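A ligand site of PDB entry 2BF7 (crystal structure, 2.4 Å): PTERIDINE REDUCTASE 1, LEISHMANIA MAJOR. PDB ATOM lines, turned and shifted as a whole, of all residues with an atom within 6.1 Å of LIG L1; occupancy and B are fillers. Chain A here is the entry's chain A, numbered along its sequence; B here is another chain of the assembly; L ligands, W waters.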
ATOM      1  N   ARG A  17      24.772 -34.995  27.099  1.00  0.00           N
ATOM      2  CA  ARG A  17      24.915 -33.788  26.284  1.00  0.00           C
ATOM      3  C   ARG A  17      26.044 -32.836  26.736  1.00  0.00           C
ATOM      4  O   ARG A  17      27.188 -33.296  26.897  1.00  0.00           O
ATOM      5  CB  ARG A  17      23.547 -33.109  26.113  1.00  0.00           C
ATOM      6  CG  ARG A  17      22.528 -34.044  25.424  1.00  0.00           C
ATOM      7  CD  ARG A  17      21.059 -33.694  25.643  1.00  0.00           C
ATOM      8  NE  ARG A  17      20.770 -32.301  25.302  1.00  0.00           N
ATOM      9  CZ  ARG A  17      20.645 -31.829  24.067  1.00  0.00           C
ATOM     10  NH1 ARG A  17      20.753 -32.634  23.004  1.00  0.00           N
ATOM     11  NH2 ARG A  17      20.406 -30.538  23.872  1.00  0.00           N
ATOM     12  N   ASN A 109      25.160 -26.431  35.433  1.00  0.00           N
ATOM     13  CA  ASN A 109      24.750 -26.826  34.079  1.00  0.00           C
ATOM     14  C   ASN A 109      23.323 -27.340  33.961  1.00  0.00           C
ATOM     15  O   ASN A 109      22.681 -27.135  32.917  1.00  0.00           O
ATOM     16  CB  ASN A 109      25.756 -27.837  33.510  1.00  0.00           C
ATOM     17  CG  ASN A 109      25.309 -28.455  32.202  1.00  0.00           C
ATOM     18  OD1 ASN A 109      25.555 -27.905  31.137  1.00  0.00           O
ATOM     19  ND2 ASN A 109      24.669 -29.617  32.280  1.00  0.00           N
ATOM     20  N   ALA A 110      22.827 -27.991  35.022  1.00  0.00           N
ATOM     21  CA  ALA A 110      21.474 -28.564  35.060  1.00  0.00           C
ATOM     22  C   ALA A 110      20.437 -27.502  34.716  1.00  0.00           C
ATOM     23  O   ALA A 110      20.552 -26.362  35.172  1.00  0.00           O
ATOM     24  CB  ALA A 110      21.173 -29.171  36.424  1.00  0.00           C
ATOM     25  N   SER A 111      19.431 -27.877  33.933  1.00  0.00           N
ATOM     26  CA  SER A 111      18.461 -26.906  33.460  1.00  0.00           C
ATOM     27  C   SER A 111      17.231 -27.535  32.817  1.00  0.00           C
ATOM     28  O   SER A 111      17.350 -28.377  31.920  1.00  0.00           O
ATOM     29  CB  SER A 111      19.175 -26.008  32.420  1.00  0.00           C
ATOM     30  OG  SER A 111      18.294 -25.299  31.581  1.00  0.00           O
ATOM     31  N   SER A 112      16.048 -27.132  33.265  1.00  0.00           N
ATOM     32  CA  SER A 112      14.823 -27.571  32.615  1.00  0.00           C
ATOM     33  C   SER A 112      14.462 -26.536  31.545  1.00  0.00           C
ATOM     34  O   SER A 112      14.810 -25.341  31.683  1.00  0.00           O
ATOM     35  CB  SER A 112      13.671 -27.786  33.604  1.00  0.00           C
ATOM     36  OG  SER A 112      13.643 -26.809  34.616  1.00  0.00           O
ATOM     37  N   PHE A 113      13.797 -26.994  30.483  1.00  0.00           N
ATOM     38  CA  PHE A 113      13.470 -26.143  29.349  1.00  0.00           C
ATOM     39  C   PHE A 113      12.191 -26.601  28.635  1.00  0.00           C
ATOM     40  O   PHE A 113      12.175 -27.619  27.960  1.00  0.00           O
ATOM     41  CB  PHE A 113      14.690 -26.101  28.413  1.00  0.00           C
ATOM     42  CG  PHE A 113      14.450 -25.464  27.062  1.00  0.00           C
ATOM     43  CD1 PHE A 113      14.521 -24.079  26.902  1.00  0.00           C
ATOM     44  CD2 PHE A 113      14.251 -26.262  25.927  1.00  0.00           C
ATOM     45  CE1 PHE A 113      14.342 -23.488  25.659  1.00  0.00           C
ATOM     46  CE2 PHE A 113      14.068 -25.684  24.669  1.00  0.00           C
ATOM     47  CZ  PHE A 113      14.100 -24.293  24.528  1.00  0.00           C
ATOM     48  N   ASN A 147      17.480 -23.545  36.948  1.00  0.00           N
ATOM     49  CA  ASN A 147      18.207 -22.489  36.242  1.00  0.00           C
ATOM     50  C   ASN A 147      18.737 -21.331  37.074  1.00  0.00           C
ATOM     51  O   ASN A 147      19.688 -20.673  36.634  1.00  0.00           O
ATOM     52  CB  ASN A 147      17.345 -21.911  35.104  1.00  0.00           C
ATOM     53  CG  ASN A 147      17.136 -22.878  33.958  1.00  0.00           C
ATOM     54  OD1 ASN A 147      18.066 -23.205  33.212  1.00  0.00           O
ATOM     55  ND2 ASN A 147      15.900 -23.359  33.813  1.00  0.00           N
ATOM     56  N   ASP A 181      22.564 -18.472  28.331  1.00  0.00           N
ATOM     57  CA  ASP A 181      21.999 -18.611  26.983  1.00  0.00           C
ATOM     58  C   ASP A 181      22.345 -17.373  26.180  1.00  0.00           C
ATOM     59  O   ASP A 181      21.945 -16.275  26.530  1.00  0.00           O
ATOM     60  CB  ASP A 181      20.482 -18.758  27.098  1.00  0.00           C
ATOM     61  CG  ASP A 181      19.805 -19.181  25.788  1.00  0.00           C
ATOM     62  OD1 ASP A 181      20.291 -18.905  24.682  1.00  0.00           O
ATOM     63  OD2 ASP A 181      18.724 -19.806  25.797  1.00  0.00           O
ATOM     64  N   LEU A 188      12.915 -16.649  22.871  1.00  0.00           N
ATOM     65  CA  LEU A 188      12.228 -17.682  22.135  1.00  0.00           C
ATOM     66  C   LEU A 188      10.740 -17.567  22.514  1.00  0.00           C
ATOM     67  O   LEU A 188      10.401 -17.506  23.704  1.00  0.00           O
ATOM     68  CB  LEU A 188      12.785 -19.045  22.513  1.00  0.00           C
ATOM     69  CG  LEU A 188      12.391 -20.274  21.692  1.00  0.00           C
ATOM     70  CD1 LEU A 188      12.609 -20.089  20.181  1.00  0.00           C
ATOM     71  CD2 LEU A 188      13.148 -21.491  22.212  1.00  0.00           C
ATOM     72  N   TYR A 194      11.631 -19.582  31.508  1.00  0.00           N
ATOM     73  CA  TYR A 194      12.974 -20.048  31.208  1.00  0.00           C
ATOM     74  C   TYR A 194      13.878 -18.840  30.974  1.00  0.00           C
ATOM     75  O   TYR A 194      14.970 -18.747  31.560  1.00  0.00           O
ATOM     76  CB  TYR A 194      12.999 -20.963  29.978  1.00  0.00           C
ATOM     77  CG  TYR A 194      14.397 -21.156  29.407  1.00  0.00           C
ATOM     78  CD1 TYR A 194      15.253 -22.133  29.917  1.00  0.00           C
ATOM     79  CD2 TYR A 194      14.868 -20.347  28.363  1.00  0.00           C
ATOM     80  CE1 TYR A 194      16.528 -22.312  29.408  1.00  0.00           C
ATOM     81  CE2 TYR A 194      16.139 -20.522  27.838  1.00  0.00           C
ATOM     82  CZ  TYR A 194      16.962 -21.505  28.362  1.00  0.00           C
ATOM     83  OH  TYR A 194      18.219 -21.663  27.840  1.00  0.00           O
ATOM     84  N   LYS A 198      17.122 -17.548  33.191  1.00  0.00           N
ATOM     85  CA  LYS A 198      18.458 -17.325  32.621  1.00  0.00           C
ATOM     86  C   LYS A 198      18.929 -15.883  32.887  1.00  0.00           C
ATOM     87  O   LYS A 198      20.122 -15.643  33.136  1.00  0.00           O
ATOM     88  CB  LYS A 198      18.504 -17.688  31.139  1.00  0.00           C
ATOM     89  CG  LYS A 198      18.412 -19.201  30.858  1.00  0.00           C
ATOM     90  CD  LYS A 198      19.481 -20.005  31.607  1.00  0.00           C
ATOM     91  CE  LYS A 198      19.758 -21.333  30.922  1.00  0.00           C
ATOM     92  NZ  LYS A 198      20.447 -22.335  31.802  1.00  0.00           N
ATOM     93  N   GLY A 225      24.373 -21.056  21.895  1.00  0.00           N
ATOM     94  CA  GLY A 225      23.311 -20.574  21.036  1.00  0.00           C
ATOM     95  C   GLY A 225      22.479 -21.801  20.718  1.00  0.00           C
ATOM     96  O   GLY A 225      21.451 -22.065  21.363  1.00  0.00           O
ATOM     97  N   LEU A 226      22.933 -22.544  19.708  1.00  0.00           N
ATOM     98  CA  LEU A 226      22.333 -23.803  19.328  1.00  0.00           C
ATOM     99  C   LEU A 226      23.417 -24.856  19.420  1.00  0.00           C
ATOM    100  O   LEU A 226      24.409 -24.780  18.693  1.00  0.00           O
ATOM    101  CB  LEU A 226      21.729 -23.768  17.919  1.00  0.00           C
ATOM    102  CG  LEU A 226      20.629 -22.731  17.642  1.00  0.00           C
ATOM    103  CD1 LEU A 226      20.154 -22.832  16.167  1.00  0.00           C
ATOM    104  CD2 LEU A 226      19.433 -22.839  18.604  1.00  0.00           C
ATOM    105  N   SER A 227      23.244 -25.794  20.345  1.00  0.00           N
ATOM    106  CA  SER A 227      24.182 -26.893  20.572  1.00  0.00           C
ATOM    107  C   SER A 227      23.453 -28.222  20.618  1.00  0.00           C
ATOM    108  O   SER A 227      22.471 -28.355  21.352  1.00  0.00           O
ATOM    109  CB  SER A 227      24.928 -26.699  21.889  1.00  0.00           C
ATOM    110  OG  SER A 227      25.808 -25.620  21.777  1.00  0.00           O
ATOM    111  N   VAL A 228      23.960 -29.195  19.868  1.00  0.00           N
ATOM    112  CA  VAL A 228      23.387 -30.537  19.787  1.00  0.00           C
ATOM    113  C   VAL A 228      21.868 -30.398  19.797  1.00  0.00           C
ATOM    114  O   VAL A 228      21.166 -30.929  20.657  1.00  0.00           O
ATOM    115  CB  VAL A 228      23.964 -31.501  20.869  1.00  0.00           C
ATOM    116  CG1 VAL A 228      25.458 -31.692  20.666  1.00  0.00           C
ATOM    117  CG2 VAL A 228      23.721 -30.982  22.280  1.00  0.00           C
ATOM    118  N   LEU A 229      21.406 -29.618  18.833  1.00  0.00           N
ATOM    119  CA  LEU A 229      19.993 -29.313  18.652  1.00  0.00           C
ATOM    120  C   LEU A 229      19.156 -30.591  18.601  1.00  0.00           C
ATOM    121  O   LEU A 229      19.453 -31.487  17.813  1.00  0.00           O
ATOM    122  CB  LEU A 229      19.824 -28.482  17.370  1.00  0.00           C
ATOM    123  CG  LEU A 229      18.491 -27.815  17.063  1.00  0.00           C
ATOM    124  CD1 LEU A 229      18.152 -26.709  18.072  1.00  0.00           C
ATOM    125  CD2 LEU A 229      18.532 -27.274  15.639  1.00  0.00           C
ATOM    126  N   VAL A 230      18.144 -30.690  19.463  1.00  0.00           N
ATOM    127  CA  VAL A 230      17.276 -31.860  19.461  1.00  0.00           C
ATOM    128  C   VAL A 230      16.600 -31.959  18.081  1.00  0.00           C
ATOM    129  O   VAL A 230      16.092 -30.966  17.556  1.00  0.00           O
ATOM    130  CB  VAL A 230      16.221 -31.845  20.589  1.00  0.00           C
ATOM    131  CG1 VAL A 230      15.430 -33.157  20.596  1.00  0.00           C
ATOM    132  CG2 VAL A 230      16.894 -31.626  21.958  1.00  0.00           C
ATOM    133  N   ARG B 287      15.266 -12.865  15.916  1.00  0.00           N
ATOM    134  CA  ARG B 287      16.401 -13.667  15.495  1.00  0.00           C
ATOM    135  C   ARG B 287      16.044 -14.246  14.140  1.00  0.00           C
ATOM    136  O   ARG B 287      14.852 -14.303  13.796  1.00  0.00           O
ATOM    137  CB  ARG B 287      16.706 -14.772  16.519  1.00  0.00           C
ATOM    138  CG  ARG B 287      15.492 -15.617  16.966  1.00  0.00           C
ATOM    139  CD  ARG B 287      15.877 -16.863  17.751  1.00  0.00           C
ATOM    140  NE  ARG B 287      15.873 -16.641  19.196  1.00  0.00           N
ATOM    141  CZ  ARG B 287      16.129 -17.572  20.106  1.00  0.00           C
ATOM    142  NH1 ARG B 287      16.428 -18.814  19.735  1.00  0.00           N
ATOM    143  NH2 ARG B 287      16.080 -17.267  21.394  1.00  0.00           N
HETATM  144  N1  LIG L   1      18.240 -25.396  27.783  1.00  0.00           N
HETATM  145  N2  LIG L   1      18.211 -27.154  29.537  1.00  0.00           N
HETATM  146  C1  LIG L   1      18.209 -26.749  28.164  1.00  0.00           C
HETATM  147  N3  LIG L   1      18.168 -27.719  27.193  1.00  0.00           N
HETATM  148  C2  LIG L   1      18.166 -27.417  25.842  1.00  0.00           C
HETATM  149  O1  LIG L   1      18.127 -28.495  24.954  1.00  0.00           O
HETATM  150  C3  LIG L   1      18.206 -26.029  25.388  1.00  0.00           C
HETATM  151  C4  LIG L   1      18.244 -25.013  26.428  1.00  0.00           C
HETATM  152  N4  LIG L   1      18.281 -23.614  26.045  1.00  0.00           N
HETATM  153  C5  LIG L   1      18.267 -23.218  24.574  1.00  0.00           C
HETATM  154  C6  LIG L   1      18.229 -24.415  23.586  1.00  0.00           C
HETATM  155  N5  LIG L   1      18.198 -25.674  24.047  1.00  0.00           N
HETATM  156  C7  LIG L   1      18.212 -24.130  22.050  1.00  0.00           C
HETATM  157  O2  LIG L   1      19.013 -25.105  21.302  1.00  0.00           O
HETATM  158  C8  LIG L   1      16.658 -24.020  21.550  1.00  0.00           C
HETATM  159  O3  LIG L   1      16.533 -23.184  20.373  1.00  0.00           O
HETATM  160  C9  LIG L   1      15.938 -25.376  21.234  1.00  0.00           C
HETATM  161  P1  LG2 L   2      19.836 -30.415  28.819  1.00  0.00           P
HETATM  162  O1  LG2 L   2      18.518 -29.925  28.406  1.00  0.00           O
HETATM  163  O2  LG2 L   2      20.253 -31.629  28.007  1.00  0.00           O
HETATM  164  O3  LG2 L   2      19.750 -30.754  30.376  1.00  0.00           O
HETATM  165  C1  LG2 L   2      20.874 -30.943  31.177  1.00  0.00           C
HETATM  166  C2  LG2 L   2      20.421 -31.607  32.469  1.00  0.00           C
HETATM  167  O4  LG2 L   2      19.692 -30.746  33.341  1.00  0.00           O
HETATM  168  C3  LG2 L   2      19.486 -32.792  32.254  1.00  0.00           C
HETATM  169  O5  LG2 L   2      20.194 -33.928  31.824  1.00  0.00           O
HETATM  170  C4  LG2 L   2      18.846 -32.951  33.626  1.00  0.00           C
HETATM  171  O6  LG2 L   2      19.405 -34.019  34.383  1.00  0.00           O
HETATM  172  C5  LG2 L   2      19.138 -31.615  34.324  1.00  0.00           C
HETATM  173  N1  LG2 L   2      17.912 -31.088  34.934  1.00  0.00           N
HETATM  174  C6  LG2 L   2      16.801 -30.573  34.345  1.00  0.00           C
HETATM  175  N2  LG2 L   2      15.917 -30.225  35.306  1.00  0.00           N
HETATM  176  C7  LG2 L   2      16.436 -30.524  36.510  1.00  0.00           C
HETATM  177  C8  LG2 L   2      15.983 -30.392  37.818  1.00  0.00           C
HETATM  178  N3  LG2 L   2      14.710 -30.088  38.105  1.00  0.00           N
HETATM  179  N4  LG2 L   2      16.792 -30.820  38.850  1.00  0.00           N
HETATM  180  C9  LG2 L   2      18.030 -31.358  38.618  1.00  0.00           C
HETATM  181  N5  LG2 L   2      18.474 -31.477  37.328  1.00  0.00           N
HETATM  182  C10 LG2 L   2      17.693 -31.067  36.289  1.00  0.00           C
HETATM  183  O7  LG2 L   2      20.922 -29.217  28.735  1.00  0.00           O
HETATM  184  P2  LG2 L   2      21.969 -29.010  27.507  1.00  0.00           P
HETATM  185  O8  LG2 L   2      21.176 -28.844  26.266  1.00  0.00           O
HETATM  186  O9  LG2 L   2      23.065 -30.012  27.590  1.00  0.00           O
HETATM  187  O10 LG2 L   2      22.598 -27.579  27.917  1.00  0.00           O
HETATM  188  C11 LG2 L   2      23.301 -27.425  29.131  1.00  0.00           C
HETATM  189  C12 LG2 L   2      23.218 -25.986  29.622  1.00  0.00           C
HETATM  190  O11 LG2 L   2      23.437 -25.089  28.543  1.00  0.00           O
HETATM  191  C13 LG2 L   2      21.857 -25.664  30.193  1.00  0.00           C
HETATM  192  O12 LG2 L   2      22.025 -24.839  31.325  1.00  0.00           O
HETATM  193  C14 LG2 L   2      21.186 -24.874  29.086  1.00  0.00           C
HETATM  194  O13 LG2 L   2      20.221 -23.947  29.540  1.00  0.00           O
HETATM  195  C15 LG2 L   2      22.358 -24.178  28.413  1.00  0.00           C
HETATM  196  N6  LG2 L   2      22.002 -23.932  27.007  1.00  0.00           N
HETATM  197  C16 LG2 L   2      21.938 -24.977  26.109  1.00  0.00           C
HETATM  198  C17 LG2 L   2      21.583 -24.730  24.783  1.00  0.00           C
HETATM  199  C18 LG2 L   2      21.623 -25.820  23.733  1.00  0.00           C
HETATM  200  O14 LG2 L   2      21.371 -25.454  22.409  1.00  0.00           O
HETATM  201  N7  LG2 L   2      21.919 -27.082  24.050  1.00  0.00           N
HETATM  202  C19 LG2 L   2      21.311 -23.428  24.395  1.00  0.00           C
HETATM  203  C20 LG2 L   2      21.380 -22.387  25.309  1.00  0.00           C
HETATM  204  C21 LG2 L   2      21.731 -22.647  26.621  1.00  0.00           C
HETATM  205  P3  LG2 L   2      18.811 -35.520  34.353  1.00  0.00           P
HETATM  206  O15 LG2 L   2      19.639 -36.352  35.262  1.00  0.00           O
HETATM  207  O16 LG2 L   2      17.373 -35.558  34.882  1.00  0.00           O
HETATM  208  O17 LG2 L   2      18.857 -36.064  32.923  1.00  0.00           O
HETATM  209  O   HOH W   1      17.129 -20.676  21.625  1.00  0.00           O
HETATM  210  O   HOH W   2      18.119 -28.395  21.473  1.00  0.00           O
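O4 of LG2 L2 sits at hydrogen-bond distance from N of Ser 111, 2.9 Å away.
An oxygen (O14) of LG2 L2 lies within hydrogen-bond range of the backbone NH (N) of Ser 227 (2.8 Å).
The backbone carbonyl oxygen (O) of Ser 111 is in hydrogen-bond range of a nitrogen (N2) of LIG L1, 2.8 Å away.
A nitrogen (N4) of LIG L1 is in hydrogen-bond range of the side-chain hydroxyl (OH) of Tyr 194.
OG of Ser 111 lies within hydrogen-bond range of O13 of LG2 L2, 3.1 Å away.
The guanidinium group of Arg 17 is in hydrogen-bond range of an oxygen (O1) of LIG L1 (3.2 Å).
A nitrogen (N2) of LIG L1 sits at hydrogen-bond distance from the side-chain hydroxyl (OG) of Ser 111 (2.8 Å).
The guanidinium group (NE) of Arg 17 lies within salt-bridge range of an oxygen (O2) of LG2 L2, 2.8 Å away.
O of Ser 227 lies within hydrogen-bond range of N7 of LG2 L2 (3.0 Å).
O of Asn 109 lies within hydrogen-bond range of O12 of LG2 L2, at 2.9 Å.
The side-chain hydroxyl (OH) of Tyr 194 is in hydrogen-bond range of an oxygen (O13) of LG2 L2, at 3.5 Å.
The side-chain amino group (NZ) of Lys 198 is in hydrogen-bond range of an oxygen (O13) of LG2 L2.
O1 of LG2 L2 sits at hydrogen-bond distance from N3 of LIG L1 (2.5 Å).
NH1 of Arg 17 lies within hydrogen-bond range of O of Val 228, at 2.9 Å.
The side-chain hydroxyl (OG) of Ser 111 lies within hydrogen-bond range of the side-chain amide oxygen (OD1) of Asn 147 (2.7 Å).
The side-chain hydroxyl (OH) of Tyr 194 sits at hydrogen-bond distance from the side-chain carboxylate (OD2) of Asp 181.
Residues that only touch LIG L1: Phe 113 (3.6 Å), Asp 181 (3.7 Å), Gly 225 (3.9 Å), Leu 226 (3.4 Å) and Leu 229 (3.7 Å).
Along chain A the residues within 4 Å of LIG L1 span positions 17 to 229.
Water W1 lies within hydrogen-bond range of the guanidinium group of Arg 287 of chain B and an oxygen (O3) of LIG L1.
Water W2 lies within hydrogen-bond range of N of Val 230 and O2 of LIG L1.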
